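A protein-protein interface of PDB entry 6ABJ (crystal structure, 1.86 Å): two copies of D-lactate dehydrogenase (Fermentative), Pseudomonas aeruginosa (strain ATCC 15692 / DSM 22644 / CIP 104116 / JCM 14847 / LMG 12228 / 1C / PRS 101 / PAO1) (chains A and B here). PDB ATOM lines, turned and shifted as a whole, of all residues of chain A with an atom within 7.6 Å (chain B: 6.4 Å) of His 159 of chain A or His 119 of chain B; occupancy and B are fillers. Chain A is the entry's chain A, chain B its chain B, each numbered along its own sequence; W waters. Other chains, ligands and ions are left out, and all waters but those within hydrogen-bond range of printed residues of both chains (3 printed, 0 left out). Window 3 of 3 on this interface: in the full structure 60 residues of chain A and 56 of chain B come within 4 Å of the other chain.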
ATOM      1  N   ASN A 133      -6.358   6.649 -19.947  1.00  0.00           N
ATOM      2  CA  ASN A 133      -6.952   7.105 -18.670  1.00  0.00           C
ATOM      3  C   ASN A 133      -7.190   5.910 -17.768  1.00  0.00           C
ATOM      4  O   ASN A 133      -6.772   5.884 -16.621  1.00  0.00           O
ATOM      5  CB  ASN A 133      -8.247   7.816 -19.017  1.00  0.00           C
ATOM      6  CG  ASN A 133      -8.996   8.364 -17.833  1.00  0.00           C
ATOM      7  OD1 ASN A 133      -8.874   7.886 -16.741  1.00  0.00           O
ATOM      8  ND2 ASN A 133      -9.787   9.386 -18.079  1.00  0.00           N
ATOM      9  N   ARG A 134      -7.901   4.935 -18.305  1.00  0.00           N
ATOM     10  CA  ARG A 134      -8.283   3.800 -17.506  1.00  0.00           C
ATOM     11  C   ARG A 134      -7.299   2.646 -17.566  1.00  0.00           C
ATOM     12  O   ARG A 134      -7.542   1.579 -16.998  1.00  0.00           O
ATOM     13  CB  ARG A 134      -9.692   3.326 -17.892  1.00  0.00           C
ATOM     14  CG  ARG A 134     -10.743   4.430 -17.913  1.00  0.00           C
ATOM     15  CD  ARG A 134     -10.810   5.154 -16.577  1.00  0.00           C
ATOM     16  NE  ARG A 134     -11.398   4.301 -15.551  1.00  0.00           N
ATOM     17  CZ  ARG A 134     -12.658   4.385 -15.137  1.00  0.00           C
ATOM     18  NH1 ARG A 134     -13.470   5.298 -15.652  1.00  0.00           N
ATOM     19  NH2 ARG A 134     -13.106   3.557 -14.207  1.00  0.00           N
ATOM     20  N   PHE A 156      -9.174   8.926 -14.070  1.00  0.00           N
ATOM     21  CA  PHE A 156      -9.837  10.160 -13.758  1.00  0.00           C
ATOM     22  C   PHE A 156     -11.094  10.287 -14.566  1.00  0.00           C
ATOM     23  O   PHE A 156     -11.148   9.893 -15.731  1.00  0.00           O
ATOM     24  CB  PHE A 156      -8.910  11.399 -13.994  1.00  0.00           C
ATOM     25  CG  PHE A 156      -8.426  11.596 -15.474  1.00  0.00           C
ATOM     26  CD1 PHE A 156      -7.240  11.016 -15.922  1.00  0.00           C
ATOM     27  CD2 PHE A 156      -9.086  12.438 -16.340  1.00  0.00           C
ATOM     28  CE1 PHE A 156      -6.781  11.204 -17.225  1.00  0.00           C
ATOM     29  CE2 PHE A 156      -8.637  12.637 -17.662  1.00  0.00           C
ATOM     30  CZ  PHE A 156      -7.463  12.006 -18.104  1.00  0.00           C
ATOM     31  N   ASP A 157     -12.122  10.881 -13.973  1.00  0.00           N
ATOM     32  CA  ASP A 157     -13.331  11.163 -14.725  1.00  0.00           C
ATOM     33  C   ASP A 157     -13.028  12.177 -15.821  1.00  0.00           C
ATOM     34  O   ASP A 157     -12.331  13.165 -15.599  1.00  0.00           O
ATOM     35  CB  ASP A 157     -14.420  11.779 -13.854  1.00  0.00           C
ATOM     36  CG  ASP A 157     -14.898  10.859 -12.741  1.00  0.00           C
ATOM     37  OD1 ASP A 157     -14.435   9.701 -12.652  1.00  0.00           O
ATOM     38  OD2 ASP A 157     -15.751  11.326 -11.956  1.00  0.00           O
ATOM     39  N   LEU A 158     -13.594  11.934 -16.990  1.00  0.00           N
ATOM     40  CA  LEU A 158     -13.523  12.883 -18.070  1.00  0.00           C
ATOM     41  C   LEU A 158     -14.485  14.047 -17.835  1.00  0.00           C
ATOM     42  O   LEU A 158     -14.185  15.212 -18.160  1.00  0.00           O
ATOM     43  CB  LEU A 158     -13.896  12.228 -19.414  1.00  0.00           C
ATOM     44  CG  LEU A 158     -12.860  11.251 -19.940  1.00  0.00           C
ATOM     45  CD1 LEU A 158     -13.335  10.598 -21.263  1.00  0.00           C
ATOM     46  CD2 LEU A 158     -11.488  11.850 -20.197  1.00  0.00           C
ATOM     47  N   HIS A 159     -15.652  13.698 -17.293  1.00  0.00           N
ATOM     48  CA  HIS A 159     -16.647  14.722 -16.938  1.00  0.00           C
ATOM     49  C   HIS A 159     -15.990  15.862 -16.168  1.00  0.00           C
ATOM     50  O   HIS A 159     -15.270  15.620 -15.201  1.00  0.00           O
ATOM     51  CB  HIS A 159     -17.711  14.101 -16.067  1.00  0.00           C
ATOM     52  CG  HIS A 159     -18.829  15.031 -15.745  1.00  0.00           C
ATOM     53  ND1 HIS A 159     -19.024  15.536 -14.481  1.00  0.00           N
ATOM     54  CD2 HIS A 159     -19.805  15.557 -16.515  1.00  0.00           C
ATOM     55  CE1 HIS A 159     -20.070  16.343 -14.481  1.00  0.00           C
ATOM     56  NE2 HIS A 159     -20.583  16.347 -15.700  1.00  0.00           N
ATOM     57  N   GLY A 160     -16.158  17.086 -16.651  1.00  0.00           N
ATOM     58  CA  GLY A 160     -15.634  18.266 -15.904  1.00  0.00           C
ATOM     59  C   GLY A 160     -14.241  18.688 -16.371  1.00  0.00           C
ATOM     60  O   GLY A 160     -13.789  19.807 -16.070  1.00  0.00           O
ATOM     61  N   LYS A 161     -13.499  17.789 -17.041  1.00  0.00           N
ATOM     62  CA  LYS A 161     -12.152  18.142 -17.417  1.00  0.00           C
ATOM     63  C   LYS A 161     -12.122  19.095 -18.610  1.00  0.00           C
ATOM     64  O   LYS A 161     -12.998  19.087 -19.452  1.00  0.00           O
ATOM     65  CB  LYS A 161     -11.266  16.895 -17.678  1.00  0.00           C
ATOM     66  CG  LYS A 161     -11.121  15.912 -16.527  1.00  0.00           C
ATOM     67  CD  LYS A 161     -10.477  16.576 -15.307  1.00  0.00           C
ATOM     68  CE  LYS A 161     -10.217  15.643 -14.151  1.00  0.00           C
ATOM     69  NZ  LYS A 161     -11.437  14.917 -13.726  1.00  0.00           N
ATOM     70  N   ARG A 162     -11.044  19.859 -18.703  1.00  0.00           N
ATOM     71  CA  ARG A 162     -10.782  20.739 -19.817  1.00  0.00           C
ATOM     72  C   ARG A 162     -10.067  20.010 -20.935  1.00  0.00           C
ATOM     73  O   ARG A 162      -9.005  19.471 -20.716  1.00  0.00           O
ATOM     74  CB  ARG A 162      -9.895  21.911 -19.364  1.00  0.00           C
ATOM     75  CG  ARG A 162     -10.683  22.806 -18.435  1.00  0.00           C
ATOM     76  CD  ARG A 162      -9.821  23.726 -17.581  1.00  0.00           C
ATOM     77  NE  ARG A 162     -10.742  24.408 -16.682  1.00  0.00           N
ATOM     78  CZ  ARG A 162     -10.386  25.000 -15.557  1.00  0.00           C
ATOM     79  NH1 ARG A 162      -9.112  25.005 -15.201  1.00  0.00           N
ATOM     80  NH2 ARG A 162     -11.307  25.599 -14.808  1.00  0.00           N
ATOM     81  N   MET A 179     -16.387  14.909 -27.185  1.00  0.00           N
ATOM     82  CA  MET A 179     -15.893  15.175 -25.836  1.00  0.00           C
ATOM     83  C   MET A 179     -16.863  16.052 -25.019  1.00  0.00           C
ATOM     84  O   MET A 179     -16.989  15.888 -23.793  1.00  0.00           O
ATOM     85  CB  MET A 179     -14.502  15.794 -25.871  1.00  0.00           C
ATOM     86  CG  MET A 179     -13.416  14.885 -26.480  1.00  0.00           C
ATOM     87  SD  MET A 179     -13.316  13.240 -25.662  1.00  0.00           S
ATOM     88  CE  MET A 179     -12.611  13.644 -24.118  1.00  0.00           C
ATOM     89  N   ALA A 180     -17.586  16.892 -25.721  1.00  0.00           N
ATOM     90  CA  ALA A 180     -18.679  17.687 -25.068  1.00  0.00           C
ATOM     91  C   ALA A 180     -19.739  16.781 -24.486  1.00  0.00           C
ATOM     92  O   ALA A 180     -20.212  17.040 -23.403  1.00  0.00           O
ATOM     93  CB  ALA A 180     -19.284  18.649 -26.057  1.00  0.00           C
ATOM     94  N   GLY A 181     -20.017  15.641 -25.140  1.00  0.00           N
ATOM     95  CA  GLY A 181     -21.023  14.699 -24.637  1.00  0.00           C
ATOM     96  C   GLY A 181     -20.622  13.970 -23.392  1.00  0.00           C
ATOM     97  O   GLY A 181     -21.481  13.457 -22.710  1.00  0.00           O
ATOM     98  N   PHE A 182     -19.320  13.913 -23.115  1.00  0.00           N
ATOM     99  CA  PHE A 182     -18.810  13.410 -21.863  1.00  0.00           C
ATOM    100  C   PHE A 182     -18.974  14.456 -20.737  1.00  0.00           C
ATOM    101  O   PHE A 182     -18.691  14.165 -19.576  1.00  0.00           O
ATOM    102  CB  PHE A 182     -17.339  13.088 -21.964  1.00  0.00           C
ATOM    103  CG  PHE A 182     -17.002  11.776 -22.633  1.00  0.00           C
ATOM    104  CD1 PHE A 182     -16.995  10.599 -21.890  1.00  0.00           C
ATOM    105  CD2 PHE A 182     -16.712  11.728 -23.986  1.00  0.00           C
ATOM    106  CE1 PHE A 182     -16.684   9.365 -22.484  1.00  0.00           C
ATOM    107  CE2 PHE A 182     -16.363  10.458 -24.584  1.00  0.00           C
ATOM    108  CZ  PHE A 182     -16.338   9.326 -23.795  1.00  0.00           C
ATOM    109  N   GLY A 183     -19.389  15.682 -21.075  1.00  0.00           N
ATOM    110  CA  GLY A 183     -19.459  16.757 -20.031  1.00  0.00           C
ATOM    111  C   GLY A 183     -18.102  17.392 -19.783  1.00  0.00           C
ATOM    112  O   GLY A 183     -17.831  17.948 -18.705  1.00  0.00           O
ATOM    113  N   CYS A 184     -17.223  17.340 -20.797  1.00  0.00           N
ATOM    114  CA  CYS A 184     -15.961  18.029 -20.733  1.00  0.00           C
ATOM    115  C   CYS A 184     -16.174  19.509 -21.025  1.00  0.00           C
ATOM    116  O   CYS A 184     -17.143  19.901 -21.685  1.00  0.00           O
ATOM    117  CB  CYS A 184     -14.970  17.458 -21.753  1.00  0.00           C
ATOM    118  SG  CYS A 184     -14.609  15.729 -21.423  1.00  0.00           S
ATOM    119  N   GLU A 185     -15.235  20.330 -20.522  1.00  0.00           N
ATOM    120  CA  GLU A 185     -15.210  21.742 -20.845  1.00  0.00           C
ATOM    121  C   GLU A 185     -14.280  21.905 -22.014  1.00  0.00           C
ATOM    122  O   GLU A 185     -13.085  21.625 -21.871  1.00  0.00           O
ATOM    123  CB  GLU A 185     -14.648  22.498 -19.614  1.00  0.00           C
ATOM    124  CG  GLU A 185     -14.568  23.988 -19.805  1.00  0.00           C
ATOM    125  CD  GLU A 185     -14.024  24.743 -18.616  1.00  0.00           C
ATOM    126  OE1 GLU A 185     -13.857  24.194 -17.500  1.00  0.00           O
ATOM    127  OE2 GLU A 185     -13.663  25.910 -18.876  1.00  0.00           O
ATOM    128  N   TYR B 116     -22.065   3.669  -6.945  1.00  0.00           N
ATOM    129  CA  TYR B 116     -20.818   4.221  -7.414  1.00  0.00           C
ATOM    130  C   TYR B 116     -21.083   5.375  -8.348  1.00  0.00           C
ATOM    131  O   TYR B 116     -22.169   5.471  -8.923  1.00  0.00           O
ATOM    132  CB  TYR B 116     -20.029   3.139  -8.151  1.00  0.00           C
ATOM    133  CG  TYR B 116     -19.613   1.969  -7.264  1.00  0.00           C
ATOM    134  CD1 TYR B 116     -18.853   2.183  -6.132  1.00  0.00           C
ATOM    135  CD2 TYR B 116     -20.014   0.659  -7.544  1.00  0.00           C
ATOM    136  CE1 TYR B 116     -18.461   1.135  -5.323  1.00  0.00           C
ATOM    137  CE2 TYR B 116     -19.654  -0.374  -6.697  1.00  0.00           C
ATOM    138  CZ  TYR B 116     -18.874  -0.120  -5.601  1.00  0.00           C
ATOM    139  OH  TYR B 116     -18.493  -1.144  -4.762  1.00  0.00           O
ATOM    140  N   SER B 117     -20.117   6.284  -8.453  1.00  0.00           N
ATOM    141  CA  SER B 117     -20.137   7.411  -9.379  1.00  0.00           C
ATOM    142  C   SER B 117     -20.584   7.017 -10.794  1.00  0.00           C
ATOM    143  O   SER B 117     -19.931   6.170 -11.461  1.00  0.00           O
ATOM    144  CB  SER B 117     -18.721   7.971  -9.498  1.00  0.00           C
ATOM    145  OG  SER B 117     -18.549   8.830 -10.619  1.00  0.00           O
ATOM    146  N   PRO B 118     -21.645   7.651 -11.283  1.00  0.00           N
ATOM    147  CA  PRO B 118     -22.179   7.234 -12.565  1.00  0.00           C
ATOM    148  C   PRO B 118     -21.281   7.644 -13.705  1.00  0.00           C
ATOM    149  O   PRO B 118     -21.194   6.893 -14.663  1.00  0.00           O
ATOM    150  CB  PRO B 118     -23.539   7.942 -12.645  1.00  0.00           C
ATOM    151  CG  PRO B 118     -23.456   9.072 -11.642  1.00  0.00           C
ATOM    152  CD  PRO B 118     -22.555   8.599 -10.577  1.00  0.00           C
ATOM    153  N   HIS B 119     -20.623   8.791 -13.632  1.00  0.00           N
ATOM    154  CA  HIS B 119     -19.674   9.129 -14.695  1.00  0.00           C
ATOM    155  C   HIS B 119     -18.498   8.163 -14.788  1.00  0.00           C
ATOM    156  O   HIS B 119     -18.117   7.769 -15.888  1.00  0.00           O
ATOM    157  CB  HIS B 119     -19.174  10.551 -14.570  1.00  0.00           C
ATOM    158  CG  HIS B 119     -20.227  11.545 -14.874  1.00  0.00           C
ATOM    159  ND1 HIS B 119     -20.632  11.820 -16.157  1.00  0.00           N
ATOM    160  CD2 HIS B 119     -21.010  12.302 -14.055  1.00  0.00           C
ATOM    161  CE1 HIS B 119     -21.611  12.715 -16.125  1.00  0.00           C
ATOM    162  NE2 HIS B 119     -21.852  13.021 -14.863  1.00  0.00           N
ATOM    163  N   ALA B 120     -17.921   7.799 -13.660  1.00  0.00           N
ATOM    164  CA  ALA B 120     -16.788   6.877 -13.679  1.00  0.00           C
ATOM    165  C   ALA B 120     -17.174   5.568 -14.343  1.00  0.00           C
ATOM    166  O   ALA B 120     -16.429   5.054 -15.218  1.00  0.00           O
ATOM    167  CB  ALA B 120     -16.254   6.625 -12.291  1.00  0.00           C
ATOM    168  N   VAL B 121     -18.316   5.007 -13.937  1.00  0.00           N
ATOM    169  CA  VAL B 121     -18.755   3.715 -14.425  1.00  0.00           C
ATOM    170  C   VAL B 121     -19.176   3.764 -15.901  1.00  0.00           C
ATOM    171  O   VAL B 121     -18.788   2.908 -16.698  1.00  0.00           O
ATOM    172  CB  VAL B 121     -19.846   3.073 -13.514  1.00  0.00           C
ATOM    173  CG1 VAL B 121     -20.272   1.705 -14.058  1.00  0.00           C
ATOM    174  CG2 VAL B 121     -19.287   2.877 -12.106  1.00  0.00           C
ATOM    175  N   ALA B 122     -19.910   4.790 -16.303  1.00  0.00           N
ATOM    176  CA  ALA B 122     -20.361   4.869 -17.681  1.00  0.00           C
ATOM    177  C   ALA B 122     -19.145   5.138 -18.640  1.00  0.00           C
ATOM    178  O   ALA B 122     -19.107   4.623 -19.740  1.00  0.00           O
ATOM    179  CB  ALA B 122     -21.403   5.967 -17.826  1.00  0.00           C
ATOM    180  N   GLU B 123     -18.201   5.946 -18.187  1.00  0.00           N
ATOM    181  CA  GLU B 123     -16.993   6.205 -18.923  1.00  0.00           C
ATOM    182  C   GLU B 123     -16.198   4.904 -19.168  1.00  0.00           C
ATOM    183  O   GLU B 123     -15.668   4.681 -20.268  1.00  0.00           O
ATOM    184  CB  GLU B 123     -16.184   7.307 -18.283  1.00  0.00           C
ATOM    185  CG  GLU B 123     -16.832   8.685 -18.465  1.00  0.00           C
ATOM    186  CD  GLU B 123     -16.081   9.790 -17.740  1.00  0.00           C
ATOM    187  OE1 GLU B 123     -14.928   9.577 -17.373  1.00  0.00           O
ATOM    188  OE2 GLU B 123     -16.695  10.889 -17.540  1.00  0.00           O
ATOM    189  N   HIS B 124     -16.146   4.060 -18.158  1.00  0.00           N
ATOM    190  CA  HIS B 124     -15.430   2.828 -18.254  1.00  0.00           C
ATOM    191  C   HIS B 124     -16.102   1.895 -19.273  1.00  0.00           C
ATOM    192  O   HIS B 124     -15.418   1.271 -20.064  1.00  0.00           O
ATOM    193  CB  HIS B 124     -15.371   2.146 -16.929  1.00  0.00           C
ATOM    194  CG  HIS B 124     -14.419   0.979 -16.921  1.00  0.00           C
ATOM    195  ND1 HIS B 124     -13.071   1.143 -16.782  1.00  0.00           N
ATOM    196  CD2 HIS B 124     -14.627  -0.349 -16.961  1.00  0.00           C
ATOM    197  CE1 HIS B 124     -12.467  -0.040 -16.784  1.00  0.00           C
ATOM    198  NE2 HIS B 124     -13.397  -0.967 -16.876  1.00  0.00           N
ATOM    199  N   ILE B 171     -26.757   5.341 -14.014  1.00  0.00           N
ATOM    200  CA  ILE B 171     -25.558   4.972 -14.788  1.00  0.00           C
ATOM    201  C   ILE B 171     -25.982   4.778 -16.250  1.00  0.00           C
ATOM    202  O   ILE B 171     -25.343   5.310 -17.166  1.00  0.00           O
ATOM    203  CB  ILE B 171     -24.863   3.739 -14.203  1.00  0.00           C
ATOM    204  CG1 ILE B 171     -24.390   3.989 -12.776  1.00  0.00           C
ATOM    205  CG2 ILE B 171     -23.617   3.431 -15.061  1.00  0.00           C
ATOM    206  CD1 ILE B 171     -23.868   2.769 -12.035  1.00  0.00           C
ATOM    207  N   THR B 174     -26.499   8.081 -17.914  1.00  0.00           N
ATOM    208  CA  THR B 174     -25.227   8.738 -18.127  1.00  0.00           C
ATOM    209  C   THR B 174     -24.523   8.125 -19.340  1.00  0.00           C
ATOM    210  O   THR B 174     -23.988   8.831 -20.207  1.00  0.00           O
ATOM    211  CB  THR B 174     -24.334   8.605 -16.880  1.00  0.00           C
ATOM    212  OG1 THR B 174     -25.060   9.046 -15.709  1.00  0.00           O
ATOM    213  CG2 THR B 174     -23.037   9.407 -17.021  1.00  0.00           C
ATOM    214  N   ARG B 177     -26.255   9.230 -22.577  1.00  0.00           N
ATOM    215  CA  ARG B 177     -25.930  10.581 -23.011  1.00  0.00           C
ATOM    216  C   ARG B 177     -24.569  10.618 -23.700  1.00  0.00           C
ATOM    217  O   ARG B 177     -24.349  11.290 -24.725  1.00  0.00           O
ATOM    218  CB  ARG B 177     -25.925  11.582 -21.796  1.00  0.00           C
ATOM    219  CG  ARG B 177     -25.560  13.029 -22.153  1.00  0.00           C
ATOM    220  CD  ARG B 177     -26.225  14.103 -21.234  1.00  0.00           C
ATOM    221  NE  ARG B 177     -26.447  13.554 -19.905  1.00  0.00           N
ATOM    222  CZ  ARG B 177     -27.619  13.178 -19.389  1.00  0.00           C
ATOM    223  NH1 ARG B 177     -28.737  13.349 -20.031  1.00  0.00           N
ATOM    224  NH2 ARG B 177     -27.655  12.601 -18.188  1.00  0.00           N
ATOM    225  N   ILE B 178     -23.602   9.895 -23.146  1.00  0.00           N
ATOM    226  CA  ILE B 178     -22.285   9.838 -23.811  1.00  0.00           C
ATOM    227  C   ILE B 178     -22.419   9.229 -25.180  1.00  0.00           C
ATOM    228  O   ILE B 178     -21.888   9.769 -26.130  1.00  0.00           O
ATOM    229  CB  ILE B 178     -21.278   9.013 -23.010  1.00  0.00           C
ATOM    230  CG1 ILE B 178     -20.996   9.682 -21.672  1.00  0.00           C
ATOM    231  CG2 ILE B 178     -19.964   8.947 -23.763  1.00  0.00           C
ATOM    232  CD1 ILE B 178     -20.269   8.793 -20.684  1.00  0.00           C
ATOM    233  N   ALA B 313     -14.505  -0.284 -12.818  1.00  0.00           N
ATOM    234  CA  ALA B 313     -15.312   0.802 -13.399  1.00  0.00           C
ATOM    235  C   ALA B 313     -15.474   2.020 -12.502  1.00  0.00           C
ATOM    236  O   ALA B 313     -15.584   3.116 -13.014  1.00  0.00           O
ATOM    237  CB  ALA B 313     -16.699   0.306 -13.813  1.00  0.00           C
ATOM    238  N   GLU B 318     -11.836  10.572  -8.484  1.00  0.00           N
ATOM    239  CA  GLU B 318     -13.064  11.186  -8.063  1.00  0.00           C
ATOM    240  C   GLU B 318     -14.055  10.179  -7.502  1.00  0.00           C
ATOM    241  O   GLU B 318     -14.738  10.438  -6.499  1.00  0.00           O
ATOM    242  CB  GLU B 318     -13.669  11.974  -9.211  1.00  0.00           C
ATOM    243  CG  GLU B 318     -12.774  13.129  -9.685  1.00  0.00           C
ATOM    244  CD  GLU B 318     -11.744  12.731 -10.767  1.00  0.00           C
ATOM    245  OE1 GLU B 318     -11.638  11.535 -11.144  1.00  0.00           O
ATOM    246  OE2 GLU B 318     -11.019  13.616 -11.245  1.00  0.00           O
HETATM  247  O   HOH W   1     -18.949  11.594 -18.565  1.00  0.00           O
HETATM  248  O   HOH W   2     -16.659  10.190  -9.675  1.00  0.00           O
HETATM  249  O   HOH W   3     -13.004   7.940 -16.832  1.00  0.00           O
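NH1 of Arg 134 of chain A sits at hydrogen-bond distance from O of Ala 120 of chain B (3.0 Å).
O of Ala 313 of chain B lies within hydrogen-bond range of NH2 of Arg 134 of chain A, at 2.8 Å.
N of Leu 158 of chain A sits at hydrogen-bond distance from OE1 of Glu 123 of chain B, at 2.7 Å.
N of His 159 of chain A lies within hydrogen-bond range of OE2 of Glu 123 of chain B.
The side-chain amino group (NZ) of Lys 161 of chain A lies within salt-bridge range of the side-chain carboxylate (OE2) of Glu 318 of chain B, at 2.8 Å.
OE1 of Glu 318 of chain B is in hydrogen-bond range of N of Asp 157 of chain A.
OG of Ser 117 of chain B lies within hydrogen-bond range of N of Ala 120 of chain B (3.3 Å).
The side-chain amide nitrogen (ND2) of Asn 133 of chain A lies within hydrogen-bond range of the backbone carbonyl oxygen (O) of Phe 156 of chain A, at 2.8 Å.
The backbone carbonyl oxygen of Lys 161 of chain A lies within hydrogen-bond range of the backbone NH of Glu 185 of chain A, 2.8 Å away.
O of Asp 157 of chain A sits at hydrogen-bond distance from NZ of Lys 161 of chain A (2.7 Å).
O of Ala 313 of chain B is in hydrogen-bond range of N of Val 121 of chain B.
The backbone carbonyl oxygen of Leu 158 of chain A sits at hydrogen-bond distance from the side-chain sulfur of Cys 184 of chain A, 3.3 Å away.
Among the printed residues, pairs that only touch across the chains: His 159 of chain A with His 119 of chain B, Phe 156 of chain A with Glu 318 of chain B, Asp 157 of chain A with Glu 123 of chain B, Arg 134 of chain A with His 124 of chain B, Phe 182 of chain A with Ile 178 of chain B, Asp 157 of chain A with Ala 120 of chain B, Gly 181 of chain A with Ile 178 of chain B, Phe 182 of chain A with Glu 123 of chain B and Asp 157 of chain A with Ser 117 of chain B.
Printed residues of chain B within 4 Å of Arg 134 of chain A: Ala 120 (3.0 Å), His 124 (3.5 Å) and Ala 313 (2.8 Å).
Of the printed residues of chain B, Leu 158 of chain A touches Glu 123 (2.7 Å).
Of chain B, only His 119 (3.4 Å) and Glu 123 (3.0 Å) come within 4 Å of His 159 of chain A.
Pro 118 of chain B touches none of the printed residues of chain A.
His 119 of chain B touches just one residue of chain A: His 159 (3.4 Å).
Of the printed residues of chain A, Ile 178 of chain B touches Gly 181 and Phe 182.
The nearest residue of chain B that does not touch His 159 of chain A is Glu 318 of chain B (6.1 Å).
The nearest residue of chain A that does not touch His 119 of chain B is Asp 157 of chain A (4.4 Å).
Of the 15 printed residues of chain B, 8 touch a printed residue of chain A.
Printed residues of chain A that touch a printed residue of chain B: Arg 134, Phe 156, Asp 157, Leu 158, His 159, Lys 161, Gly 181 and Phe 182.
Among the printed residues, 15 pairs touch across the chains.
Among the printed residues, Asp or Glu carboxylates within 4 Å of a Lys or Arg side-chain nitrogen of the other chain: Lys 161 of chain A with Glu 318 of chain B (2.8 Å).
No position is printed for both chains.
Of the 15 pairs that touch across the chains among the printed residues, none has its exchanged pair printed and touching as well.
Water W2 bridges the side-chain hydroxyl of Ser 117 of chain B (2.5 Å) and the side-chain carboxylate of Asp 157 of chain A (2.7 Å).
Water W1 lies within hydrogen-bond range of the side-chain carboxylate (OE2) of Glu 123 of chain B, the backbone carbonyl oxygen (O) of Phe 182 of chain A and a ring nitrogen (ND1) of His 119 of chain B.
Water W3 lies within hydrogen-bond range of OE1 of Glu 123 of chain B (2.6 Å), O of Phe 156 of chain A (2.9 Å) and NH1 of Arg 134 of chain A (2.9 Å).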
